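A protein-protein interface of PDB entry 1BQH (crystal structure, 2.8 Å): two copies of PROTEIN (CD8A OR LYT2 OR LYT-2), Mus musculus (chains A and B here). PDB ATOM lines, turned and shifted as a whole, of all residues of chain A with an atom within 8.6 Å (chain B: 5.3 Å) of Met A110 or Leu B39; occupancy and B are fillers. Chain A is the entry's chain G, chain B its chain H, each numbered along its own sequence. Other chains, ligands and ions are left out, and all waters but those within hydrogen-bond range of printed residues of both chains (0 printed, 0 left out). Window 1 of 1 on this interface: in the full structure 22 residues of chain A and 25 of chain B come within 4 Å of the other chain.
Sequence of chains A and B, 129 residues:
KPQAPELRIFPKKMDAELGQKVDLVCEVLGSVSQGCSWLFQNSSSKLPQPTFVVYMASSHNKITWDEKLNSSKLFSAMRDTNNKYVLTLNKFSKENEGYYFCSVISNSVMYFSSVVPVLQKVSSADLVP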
ATOM      1  N   PRO A   5     -17.839  -8.927  18.482  1.00  0.00           N
ATOM      2  CA  PRO A   5     -18.674  -7.792  18.894  1.00  0.00           C
ATOM      3  C   PRO A   5     -18.350  -6.501  18.155  1.00  0.00           C
ATOM      4  O   PRO A   5     -17.188  -6.132  18.035  1.00  0.00           O
ATOM      5  CB  PRO A   5     -18.437  -7.670  20.403  1.00  0.00           C
ATOM      6  CG  PRO A   5     -17.346  -8.631  20.749  1.00  0.00           C
ATOM      7  CD  PRO A   5     -16.990  -9.461  19.561  1.00  0.00           C
ATOM      8  N   GLU A   6     -19.384  -5.831  17.652  1.00  0.00           N
ATOM      9  CA  GLU A   6     -19.228  -4.563  16.942  1.00  0.00           C
ATOM     10  C   GLU A   6     -20.564  -3.862  16.831  1.00  0.00           C
ATOM     11  O   GLU A   6     -21.590  -4.507  16.616  1.00  0.00           O
ATOM     12  CB  GLU A   6     -18.667  -4.755  15.538  1.00  0.00           C
ATOM     13  CG  GLU A   6     -18.032  -3.472  14.981  1.00  0.00           C
ATOM     14  CD  GLU A   6     -17.222  -2.692  16.029  1.00  0.00           C
ATOM     15  OE1 GLU A   6     -16.143  -3.169  16.449  1.00  0.00           O
ATOM     16  OE2 GLU A   6     -17.667  -1.593  16.430  1.00  0.00           O
ATOM     17  N   LEU A   7     -20.537  -2.539  16.967  1.00  0.00           N
ATOM     18  CA  LEU A   7     -21.747  -1.729  16.911  1.00  0.00           C
ATOM     19  C   LEU A   7     -21.971  -0.949  15.623  1.00  0.00           C
ATOM     20  O   LEU A   7     -21.026  -0.543  14.932  1.00  0.00           O
ATOM     21  CB  LEU A   7     -21.766  -0.743  18.083  1.00  0.00           C
ATOM     22  CG  LEU A   7     -21.585  -1.337  19.480  1.00  0.00           C
ATOM     23  CD1 LEU A   7     -20.924  -0.315  20.393  1.00  0.00           C
ATOM     24  CD2 LEU A   7     -22.940  -1.752  20.026  1.00  0.00           C
ATOM     25  N   SER A  37     -23.362   1.826  26.279  1.00  0.00           N
ATOM     26  CA  SER A  37     -23.090   3.167  26.796  1.00  0.00           C
ATOM     27  C   SER A  37     -23.088   4.226  25.697  1.00  0.00           C
ATOM     28  O   SER A  37     -22.587   3.991  24.605  1.00  0.00           O
ATOM     29  CB  SER A  37     -21.732   3.190  27.505  1.00  0.00           C
ATOM     30  OG  SER A  37     -21.790   2.421  28.681  1.00  0.00           O
ATOM     31  N   LEU A  39     -21.842   7.978  24.637  1.00  0.00           N
ATOM     32  CA  LEU A  39     -20.847   9.011  24.922  1.00  0.00           C
ATOM     33  C   LEU A  39     -20.740  10.041  23.783  1.00  0.00           C
ATOM     34  O   LEU A  39     -21.071   9.730  22.644  1.00  0.00           O
ATOM     35  CB  LEU A  39     -19.500   8.300  25.171  1.00  0.00           C
ATOM     36  CG  LEU A  39     -19.671   6.905  25.808  1.00  0.00           C
ATOM     37  CD1 LEU A  39     -18.576   5.965  25.349  1.00  0.00           C
ATOM     38  CD2 LEU A  39     -19.656   7.041  27.319  1.00  0.00           C
ATOM     39  N   PRO A  50     -14.295  12.904  25.723  1.00  0.00           N
ATOM     40  CA  PRO A  50     -15.579  12.209  25.788  1.00  0.00           C
ATOM     41  C   PRO A  50     -16.206  12.292  27.163  1.00  0.00           C
ATOM     42  O   PRO A  50     -15.502  12.252  28.168  1.00  0.00           O
ATOM     43  CB  PRO A  50     -15.228  10.786  25.393  1.00  0.00           C
ATOM     44  CG  PRO A  50     -13.824  10.630  25.836  1.00  0.00           C
ATOM     45  CD  PRO A  50     -13.171  11.961  25.641  1.00  0.00           C
ATOM     46  N   PHE A 101     -21.468   8.455  19.968  1.00  0.00           N
ATOM     47  CA  PHE A 101     -21.070   7.081  19.701  1.00  0.00           C
ATOM     48  C   PHE A 101     -21.370   6.181  20.897  1.00  0.00           C
ATOM     49  O   PHE A 101     -21.182   6.569  22.044  1.00  0.00           O
ATOM     50  CB  PHE A 101     -19.578   7.026  19.376  1.00  0.00           C
ATOM     51  CG  PHE A 101     -18.691   7.549  20.475  1.00  0.00           C
ATOM     52  CD1 PHE A 101     -18.563   8.912  20.704  1.00  0.00           C
ATOM     53  CD2 PHE A 101     -17.967   6.677  21.274  1.00  0.00           C
ATOM     54  CE1 PHE A 101     -17.726   9.393  21.709  1.00  0.00           C
ATOM     55  CE2 PHE A 101     -17.131   7.157  22.277  1.00  0.00           C
ATOM     56  CZ  PHE A 101     -17.013   8.514  22.493  1.00  0.00           C
ATOM     57  N   CYS A 102     -21.842   4.977  20.623  1.00  0.00           N
ATOM     58  CA  CYS A 102     -22.155   4.042  21.689  1.00  0.00           C
ATOM     59  C   CYS A 102     -20.953   3.137  21.932  1.00  0.00           C
ATOM     60  O   CYS A 102     -20.113   2.966  21.050  1.00  0.00           O
ATOM     61  CB  CYS A 102     -23.372   3.195  21.311  1.00  0.00           C
ATOM     62  SG  CYS A 102     -23.491   2.774  19.544  1.00  0.00           S
ATOM     63  N   SER A 103     -20.866   2.557  23.124  1.00  0.00           N
ATOM     64  CA  SER A 103     -19.757   1.672  23.447  1.00  0.00           C
ATOM     65  C   SER A 103     -20.203   0.438  24.218  1.00  0.00           C
ATOM     66  O   SER A 103     -21.113   0.500  25.048  1.00  0.00           O
ATOM     67  CB  SER A 103     -18.702   2.414  24.263  1.00  0.00           C
ATOM     68  OG  SER A 103     -17.555   1.600  24.436  1.00  0.00           O
ATOM     69  N   VAL A 104     -19.550  -0.685  23.935  1.00  0.00           N
ATOM     70  CA  VAL A 104     -19.861  -1.951  24.585  1.00  0.00           C
ATOM     71  C   VAL A 104     -18.570  -2.636  25.004  1.00  0.00           C
ATOM     72  O   VAL A 104     -17.602  -2.666  24.249  1.00  0.00           O
ATOM     73  CB  VAL A 104     -20.638  -2.896  23.635  1.00  0.00           C
ATOM     74  CG1 VAL A 104     -22.099  -2.458  23.550  1.00  0.00           C
ATOM     75  CG2 VAL A 104     -19.986  -2.888  22.244  1.00  0.00           C
ATOM     76  N   ILE A 105     -18.553  -3.185  26.209  1.00  0.00           N
ATOM     77  CA  ILE A 105     -17.368  -3.860  26.692  1.00  0.00           C
ATOM     78  C   ILE A 105     -17.600  -5.362  26.757  1.00  0.00           C
ATOM     79  O   ILE A 105     -18.506  -5.832  27.451  1.00  0.00           O
ATOM     80  CB  ILE A 105     -16.990  -3.348  28.075  1.00  0.00           C
ATOM     81  CG1 ILE A 105     -16.713  -1.850  27.990  1.00  0.00           C
ATOM     82  CG2 ILE A 105     -15.762  -4.071  28.585  1.00  0.00           C
ATOM     83  CD1 ILE A 105     -16.244  -1.242  29.282  1.00  0.00           C
ATOM     84  N   SER A 106     -16.778  -6.110  26.021  1.00  0.00           N
ATOM     85  CA  SER A 106     -16.874  -7.566  25.982  1.00  0.00           C
ATOM     86  C   SER A 106     -15.562  -8.197  26.434  1.00  0.00           C
ATOM     87  O   SER A 106     -14.530  -8.009  25.798  1.00  0.00           O
ATOM     88  CB  SER A 106     -17.202  -8.036  24.564  1.00  0.00           C
ATOM     89  OG  SER A 106     -17.686  -9.366  24.578  1.00  0.00           O
ATOM     90  N   ASN A 107     -15.607  -8.944  27.537  1.00  0.00           N
ATOM     91  CA  ASN A 107     -14.421  -9.600  28.060  1.00  0.00           C
ATOM     92  C   ASN A 107     -13.328  -8.589  28.330  1.00  0.00           C
ATOM     93  O   ASN A 107     -12.177  -8.788  27.932  1.00  0.00           O
ATOM     94  CB  ASN A 107     -13.912 -10.630  27.059  1.00  0.00           C
ATOM     95  CG  ASN A 107     -14.852 -11.802  26.918  1.00  0.00           C
ATOM     96  OD1 ASN A 107     -15.409 -12.043  25.847  1.00  0.00           O
ATOM     97  ND2 ASN A 107     -15.034 -12.544  28.004  1.00  0.00           N
ATOM     98  N   SER A 108     -13.697  -7.502  29.004  1.00  0.00           N
ATOM     99  CA  SER A 108     -12.768  -6.429  29.359  1.00  0.00           C
ATOM    100  C   SER A 108     -12.149  -5.681  28.172  1.00  0.00           C
ATOM    101  O   SER A 108     -10.994  -5.244  28.241  1.00  0.00           O
ATOM    102  CB  SER A 108     -11.652  -6.986  30.248  1.00  0.00           C
ATOM    103  OG  SER A 108     -12.199  -7.554  31.427  1.00  0.00           O
ATOM    104  N   VAL A 109     -12.910  -5.531  27.091  1.00  0.00           N
ATOM    105  CA  VAL A 109     -12.414  -4.831  25.917  1.00  0.00           C
ATOM    106  C   VAL A 109     -13.441  -3.819  25.451  1.00  0.00           C
ATOM    107  O   VAL A 109     -14.541  -4.176  25.034  1.00  0.00           O
ATOM    108  CB  VAL A 109     -12.122  -5.800  24.751  1.00  0.00           C
ATOM    109  CG1 VAL A 109     -11.654  -5.016  23.542  1.00  0.00           C
ATOM    110  CG2 VAL A 109     -11.074  -6.817  25.166  1.00  0.00           C
ATOM    111  N   MET A 110     -13.077  -2.547  25.529  1.00  0.00           N
ATOM    112  CA  MET A 110     -13.976  -1.484  25.113  1.00  0.00           C
ATOM    113  C   MET A 110     -14.054  -1.442  23.603  1.00  0.00           C
ATOM    114  O   MET A 110     -13.046  -1.205  22.917  1.00  0.00           O
ATOM    115  CB  MET A 110     -13.489  -0.138  25.640  1.00  0.00           C
ATOM    116  CG  MET A 110     -13.615  -0.004  27.145  1.00  0.00           C
ATOM    117  SD  MET A 110     -13.225   1.657  27.802  1.00  0.00           S
ATOM    118  CE  MET A 110     -14.266   2.708  26.733  1.00  0.00           C
ATOM    119  N   TYR A 111     -15.261  -1.683  23.099  1.00  0.00           N
ATOM    120  CA  TYR A 111     -15.544  -1.684  21.669  1.00  0.00           C
ATOM    121  C   TYR A 111     -16.451  -0.457  21.380  1.00  0.00           C
ATOM    122  O   TYR A 111     -17.568  -0.383  21.902  1.00  0.00           O
ATOM    123  CB  TYR A 111     -16.251  -3.006  21.294  1.00  0.00           C
ATOM    124  CG  TYR A 111     -15.424  -4.289  21.496  1.00  0.00           C
ATOM    125  CD1 TYR A 111     -14.468  -4.680  20.563  1.00  0.00           C
ATOM    126  CD2 TYR A 111     -15.612  -5.110  22.612  1.00  0.00           C
ATOM    127  CE1 TYR A 111     -13.723  -5.846  20.729  1.00  0.00           C
ATOM    128  CE2 TYR A 111     -14.863  -6.286  22.783  1.00  0.00           C
ATOM    129  CZ  TYR A 111     -13.921  -6.645  21.836  1.00  0.00           C
ATOM    130  OH  TYR A 111     -13.174  -7.796  21.988  1.00  0.00           O
ATOM    131  N   PHE A 112     -15.963   0.501  20.575  1.00  0.00           N
ATOM    132  CA  PHE A 112     -16.726   1.721  20.219  1.00  0.00           C
ATOM    133  C   PHE A 112     -17.370   1.598  18.840  1.00  0.00           C
ATOM    134  O   PHE A 112     -16.906   0.826  17.995  1.00  0.00           O
ATOM    135  CB  PHE A 112     -15.837   2.979  20.155  1.00  0.00           C
ATOM    136  CG  PHE A 112     -14.981   3.197  21.356  1.00  0.00           C
ATOM    137  CD1 PHE A 112     -13.779   2.529  21.488  1.00  0.00           C
ATOM    138  CD2 PHE A 112     -15.373   4.071  22.349  1.00  0.00           C
ATOM    139  CE1 PHE A 112     -12.979   2.726  22.591  1.00  0.00           C
ATOM    140  CE2 PHE A 112     -14.582   4.275  23.458  1.00  0.00           C
ATOM    141  CZ  PHE A 112     -13.381   3.601  23.579  1.00  0.00           C
ATOM    142  N   SER A 113     -18.447   2.340  18.651  1.00  0.00           N
ATOM    143  CA  SER A 113     -19.087   2.399  17.343  1.00  0.00           C
ATOM    144  C   SER A 113     -18.420   3.439  16.450  1.00  0.00           C
ATOM    145  O   SER A 113     -17.172   3.487  16.493  1.00  0.00           O
ATOM    146  CB  SER A 113     -20.580   2.698  17.490  1.00  0.00           C
ATOM    147  OG  SER A 113     -20.791   3.975  18.066  1.00  0.00           O
ATOM    148  N   SER B  37      -8.563   1.174  32.098  1.00  0.00           N
ATOM    149  CA  SER B  37      -8.422   1.060  30.648  1.00  0.00           C
ATOM    150  C   SER B  37      -7.729   2.287  30.088  1.00  0.00           C
ATOM    151  O   SER B  37      -8.017   3.416  30.490  1.00  0.00           O
ATOM    152  CB  SER B  37      -9.791   0.918  29.977  1.00  0.00           C
ATOM    153  OG  SER B  37     -10.161  -0.445  29.888  1.00  0.00           O
ATOM    154  N   TRP B  38      -6.810   2.051  29.161  1.00  0.00           N
ATOM    155  CA  TRP B  38      -6.066   3.123  28.516  1.00  0.00           C
ATOM    156  C   TRP B  38      -6.614   3.304  27.099  1.00  0.00           C
ATOM    157  O   TRP B  38      -6.614   2.368  26.301  1.00  0.00           O
ATOM    158  CB  TRP B  38      -4.587   2.762  28.452  1.00  0.00           C
ATOM    159  CG  TRP B  38      -3.808   3.227  29.632  1.00  0.00           C
ATOM    160  CD1 TRP B  38      -3.277   2.454  30.633  1.00  0.00           C
ATOM    161  CD2 TRP B  38      -3.447   4.578  29.933  1.00  0.00           C
ATOM    162  NE1 TRP B  38      -2.605   3.247  31.534  1.00  0.00           N
ATOM    163  CE2 TRP B  38      -2.696   4.553  31.129  1.00  0.00           C
ATOM    164  CE3 TRP B  38      -3.688   5.806  29.308  1.00  0.00           C
ATOM    165  CZ2 TRP B  38      -2.177   5.709  31.707  1.00  0.00           C
ATOM    166  CZ3 TRP B  38      -3.176   6.950  29.884  1.00  0.00           C
ATOM    167  CH2 TRP B  38      -2.431   6.897  31.071  1.00  0.00           C
ATOM    168  N   LEU B  39      -7.092   4.499  26.785  1.00  0.00           N
ATOM    169  CA  LEU B  39      -7.628   4.756  25.459  1.00  0.00           C
ATOM    170  C   LEU B  39      -6.673   5.621  24.653  1.00  0.00           C
ATOM    171  O   LEU B  39      -5.700   6.172  25.190  1.00  0.00           O
ATOM    172  CB  LEU B  39      -8.975   5.454  25.566  1.00  0.00           C
ATOM    173  CG  LEU B  39     -10.049   4.622  26.248  1.00  0.00           C
ATOM    174  CD1 LEU B  39     -11.403   5.249  25.979  1.00  0.00           C
ATOM    175  CD2 LEU B  39      -9.996   3.203  25.724  1.00  0.00           C
ATOM    176  N   PHE B  40      -6.975   5.747  23.364  1.00  0.00           N
ATOM    177  CA  PHE B  40      -6.162   6.524  22.446  1.00  0.00           C
ATOM    178  C   PHE B  40      -6.994   7.091  21.305  1.00  0.00           C
ATOM    179  O   PHE B  40      -7.846   6.398  20.760  1.00  0.00           O
ATOM    180  CB  PHE B  40      -5.067   5.619  21.893  1.00  0.00           C
ATOM    181  CG  PHE B  40      -4.321   6.190  20.718  1.00  0.00           C
ATOM    182  CD1 PHE B  40      -3.708   7.431  20.798  1.00  0.00           C
ATOM    183  CD2 PHE B  40      -4.191   5.463  19.543  1.00  0.00           C
ATOM    184  CE1 PHE B  40      -2.976   7.929  19.731  1.00  0.00           C
ATOM    185  CE2 PHE B  40      -3.462   5.957  18.479  1.00  0.00           C
ATOM    186  CZ  PHE B  40      -2.854   7.189  18.573  1.00  0.00           C
ATOM    187  N   GLN B  41      -6.757   8.354  20.961  1.00  0.00           N
ATOM    188  CA  GLN B  41      -7.467   9.006  19.853  1.00  0.00           C
ATOM    189  C   GLN B  41      -6.388   9.342  18.827  1.00  0.00           C
ATOM    190  O   GLN B  41      -5.683  10.335  18.964  1.00  0.00           O
ATOM    191  CB  GLN B  41      -8.170  10.292  20.310  1.00  0.00           C
ATOM    192  CG  GLN B  41      -9.444  10.055  21.147  1.00  0.00           C
ATOM    193  CD  GLN B  41     -10.711  10.641  20.516  1.00  0.00           C
ATOM    194  OE1 GLN B  41     -11.826  10.476  21.037  1.00  0.00           O
ATOM    195  NE2 GLN B  41     -10.542  11.330  19.386  1.00  0.00           N
ATOM    196  N   PRO B  50     -12.153   7.232  19.135  1.00  0.00           N
ATOM    197  CA  PRO B  50     -11.310   6.632  20.173  1.00  0.00           C
ATOM    198  C   PRO B  50     -10.932   5.224  19.802  1.00  0.00           C
ATOM    199  O   PRO B  50     -11.675   4.521  19.121  1.00  0.00           O
ATOM    200  CB  PRO B  50     -12.161   6.653  21.436  1.00  0.00           C
ATOM    201  CG  PRO B  50     -13.500   7.177  21.039  1.00  0.00           C
ATOM    202  CD  PRO B  50     -13.520   7.527  19.594  1.00  0.00           C
ATOM    203  N   THR B  51      -9.766   4.818  20.265  1.00  0.00           N
ATOM    204  CA  THR B  51      -9.282   3.489  19.991  1.00  0.00           C
ATOM    205  C   THR B  51      -8.829   2.833  21.289  1.00  0.00           C
ATOM    206  O   THR B  51      -7.939   3.326  21.995  1.00  0.00           O
ATOM    207  CB  THR B  51      -8.100   3.510  19.002  1.00  0.00           C
ATOM    208  OG1 THR B  51      -7.046   4.335  19.525  1.00  0.00           O
ATOM    209  CG2 THR B  51      -8.548   4.049  17.650  1.00  0.00           C
ATOM    210  N   PHE B  52      -9.467   1.710  21.594  1.00  0.00           N
ATOM    211  CA  PHE B  52      -9.153   0.957  22.786  1.00  0.00           C
ATOM    212  C   PHE B  52      -7.749   0.403  22.698  1.00  0.00           C
ATOM    213  O   PHE B  52      -7.412  -0.315  21.752  1.00  0.00           O
ATOM    214  CB  PHE B  52     -10.131  -0.211  22.958  1.00  0.00           C
ATOM    215  CG  PHE B  52      -9.757  -1.156  24.083  1.00  0.00           C
ATOM    216  CD1 PHE B  52     -10.050  -0.832  25.407  1.00  0.00           C
ATOM    217  CD2 PHE B  52      -9.095  -2.353  23.826  1.00  0.00           C
ATOM    218  CE1 PHE B  52      -9.691  -1.678  26.448  1.00  0.00           C
ATOM    219  CE2 PHE B  52      -8.734  -3.199  24.858  1.00  0.00           C
ATOM    220  CZ  PHE B  52      -9.030  -2.861  26.173  1.00  0.00           C
ATOM    221  N   VAL B  53      -6.919   0.748  23.677  1.00  0.00           N
ATOM    222  CA  VAL B  53      -5.556   0.219  23.703  1.00  0.00           C
ATOM    223  C   VAL B  53      -5.570  -0.992  24.612  1.00  0.00           C
ATOM    224  O   VAL B  53      -5.568  -2.145  24.178  1.00  0.00           O
ATOM    225  CB  VAL B  53      -4.470   1.096  24.395  1.00  0.00           C
ATOM    226  CG1 VAL B  53      -3.356   0.158  24.938  1.00  0.00           C
ATOM    227  CG2 VAL B  53      -3.849   2.058  23.439  1.00  0.00           C
ATOM    228  N   TYR B  99      -3.510  11.360  20.926  1.00  0.00           N
ATOM    229  CA  TYR B  99      -3.980  11.713  22.257  1.00  0.00           C
ATOM    230  C   TYR B  99      -4.330  10.458  23.065  1.00  0.00           C
ATOM    231  O   TYR B  99      -5.091   9.598  22.613  1.00  0.00           O
ATOM    232  CB  TYR B  99      -5.214  12.623  22.156  1.00  0.00           C
ATOM    233  CG  TYR B  99      -5.104  13.765  21.156  1.00  0.00           C
ATOM    234  CD1 TYR B  99      -5.314  13.555  19.791  1.00  0.00           C
ATOM    235  CD2 TYR B  99      -4.807  15.056  21.576  1.00  0.00           C
ATOM    236  CE1 TYR B  99      -5.229  14.596  18.878  1.00  0.00           C
ATOM    237  CE2 TYR B  99      -4.721  16.102  20.668  1.00  0.00           C
ATOM    238  CZ  TYR B  99      -4.934  15.864  19.320  1.00  0.00           C
ATOM    239  OH  TYR B  99      -4.860  16.891  18.410  1.00  0.00           O
ATOM    240  N   TYR B 100      -3.771  10.369  24.267  1.00  0.00           N
ATOM    241  CA  TYR B 100      -3.999   9.226  25.144  1.00  0.00           C
ATOM    242  C   TYR B 100      -4.751   9.639  26.399  1.00  0.00           C
ATOM    243  O   TYR B 100      -4.679  10.791  26.829  1.00  0.00           O
ATOM    244  CB  TYR B 100      -2.661   8.593  25.542  1.00  0.00           C
ATOM    245  CG  TYR B 100      -1.946   7.903  24.404  1.00  0.00           C
ATOM    246  CD1 TYR B 100      -1.454   8.627  23.320  1.00  0.00           C
ATOM    247  CD2 TYR B 100      -1.772   6.532  24.403  1.00  0.00           C
ATOM    248  CE1 TYR B 100      -0.812   8.004  22.271  1.00  0.00           C
ATOM    249  CE2 TYR B 100      -1.128   5.897  23.355  1.00  0.00           C
ATOM    250  CZ  TYR B 100      -0.651   6.638  22.291  1.00  0.00           C
ATOM    251  OH  TYR B 100      -0.013   6.018  21.236  1.00  0.00           O
ATOM    252  N   PHE B 101      -5.473   8.699  26.995  1.00  0.00           N
ATOM    253  CA  PHE B 101      -6.223   9.017  28.200  1.00  0.00           C
ATOM    254  C   PHE B 101      -6.850   7.785  28.838  1.00  0.00           C
ATOM    255  O   PHE B 101      -7.344   6.908  28.142  1.00  0.00           O
ATOM    256  CB  PHE B 101      -7.307  10.038  27.868  1.00  0.00           C
ATOM    257  CG  PHE B 101      -8.433   9.491  27.038  1.00  0.00           C
ATOM    258  CD1 PHE B 101      -8.195   8.943  25.785  1.00  0.00           C
ATOM    259  CD2 PHE B 101      -9.741   9.550  27.502  1.00  0.00           C
ATOM    260  CE1 PHE B 101      -9.250   8.461  25.005  1.00  0.00           C
ATOM    261  CE2 PHE B 101     -10.795   9.072  26.730  1.00  0.00           C
ATOM    262  CZ  PHE B 101     -10.550   8.528  25.483  1.00  0.00           C
ATOM    263  N   CYS B 102      -6.833   7.722  30.165  1.00  0.00           N
ATOM    264  CA  CYS B 102      -7.400   6.573  30.849  1.00  0.00           C
ATOM    265  C   CYS B 102      -8.833   6.748  31.295  1.00  0.00           C
ATOM    266  O   CYS B 102      -9.315   7.846  31.599  1.00  0.00           O
ATOM    267  CB  CYS B 102      -6.544   6.178  32.057  1.00  0.00           C
ATOM    268  SG  CYS B 102      -6.222   7.528  33.237  1.00  0.00           S
ATOM    269  N   SER B 103      -9.491   5.602  31.330  1.00  0.00           N
ATOM    270  CA  SER B 103     -10.880   5.468  31.711  1.00  0.00           C
ATOM    271  C   SER B 103     -11.055   4.355  32.751  1.00  0.00           C
ATOM    272  O   SER B 103     -10.245   3.423  32.837  1.00  0.00           O
ATOM    273  CB  SER B 103     -11.711   5.138  30.472  1.00  0.00           C
ATOM    274  OG  SER B 103     -13.095   5.185  30.761  1.00  0.00           O
ATOM    275  N   MET B 110     -19.090   5.468  33.177  1.00  0.00           N
ATOM    276  CA  MET B 110     -17.701   5.571  32.681  1.00  0.00           C
ATOM    277  C   MET B 110     -17.050   6.923  32.924  1.00  0.00           C
ATOM    278  O   MET B 110     -17.602   7.964  32.572  1.00  0.00           O
ATOM    279  CB  MET B 110     -17.634   5.296  31.175  1.00  0.00           C
ATOM    280  CG  MET B 110     -18.144   3.943  30.770  1.00  0.00           C
ATOM    281  SD  MET B 110     -17.839   3.563  29.018  1.00  0.00           S
ATOM    282  CE  MET B 110     -16.130   4.068  28.808  1.00  0.00           C
ATOM    283  N   PHE B 112     -13.630   9.433  32.437  1.00  0.00           N
ATOM    284  CA  PHE B 112     -12.474   9.684  31.575  1.00  0.00           C
ATOM    285  C   PHE B 112     -11.587  10.833  32.095  1.00  0.00           C
ATOM    286  O   PHE B 112     -12.102  11.874  32.545  1.00  0.00           O
ATOM    287  CB  PHE B 112     -12.910  10.007  30.132  1.00  0.00           C
ATOM    288  CG  PHE B 112     -13.900   9.002  29.547  1.00  0.00           C
ATOM    289  CD1 PHE B 112     -13.431   7.876  28.864  1.00  0.00           C
ATOM    290  CD2 PHE B 112     -15.275   9.215  29.692  1.00  0.00           C
ATOM    291  CE1 PHE B 112     -14.339   6.959  28.322  1.00  0.00           C
ATOM    292  CE2 PHE B 112     -16.183   8.298  29.151  1.00  0.00           C
ATOM    293  CZ  PHE B 112     -15.715   7.171  28.466  1.00  0.00           C
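The backbone carbonyl oxygen (O) of Leu A39 lies within hydrogen-bond range of the backbone NH (N) of Phe A101 (3.0 Å).
The backbone carbonyl oxygen (O) of Phe B101 is in hydrogen-bond range of the backbone NH (N) of Leu B39 (2.8 Å).
Among the printed residues, merely in contact across the chains: Met A110 with Phe B52 (3.1 Å), Met A110 with Met B110 (3.1 Å), Pro A50 with Phe B112 (3.4 Å), Phe A112 with Leu B39 (3.5 Å), Pro A50 with Phe B101 (3.5 Å), Val A109 with Phe B52 (3.7 Å), Ser A108 with Phe B52 (3.7 Å), Phe A112 with Pro B50 (3.7 Å), Phe A112 with Phe B52 (3.8 Å), Phe A101 with Pro B50 (3.8 Å) and Met A110 with Leu B39 (3.9 Å).
Of the printed residues of chain B, Phe A101 touches Pro B50.
Printed residues of chain B within 4 Å of Met A110: Leu B39, Phe B52 and Met B110.
Of the printed residues of chain B, Phe A112 touches Leu B39, Pro B50 and Phe B52.
Leu B39 touches two residues of chain A.
Tyr B99 touches none of the printed residues of chain A.
Of the printed residues of chain A, Phe B101 touches Pro A50.
Cys B102 touches none of the printed residues of chain A.
The nearest residue of chain B that does not touch Met A110 is Ser B37 (4.1 Å).
Printed residues of chain B that touch a printed residue of chain A: Leu B39, Pro B50, Phe B52, Phe B101, Met B110 and Phe B112.
Of the 19 printed residues of chain A, 6 touch a printed residue of chain B.
Printed residues of chain A that touch a printed residue of chain B: Pro A50, Phe A101, Ser A108, Val A109, Met A110 and Phe A112.
Among the printed residues, no Asp or Glu carboxylate lies within 4 Å of a Lys or Arg side-chain nitrogen of the other chain.
Pro A50 touches Phe B101, and with the chains exchanged Phe A101 touches Pro B50.
Pro A50 touches Phe B112, and with the chains exchanged Phe A112 touches Pro B50.
Met A110 touches Leu B39, but with the chains exchanged Leu A39 does not touch Met B110 (4.3 Å).
Phe A112 touches Leu B39, but with the chains exchanged Leu A39 does not touch Phe B112 (4.1 Å).
Positions printed for both chains: 37, 39, 50, 101, 102, 103, 110 and 112.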
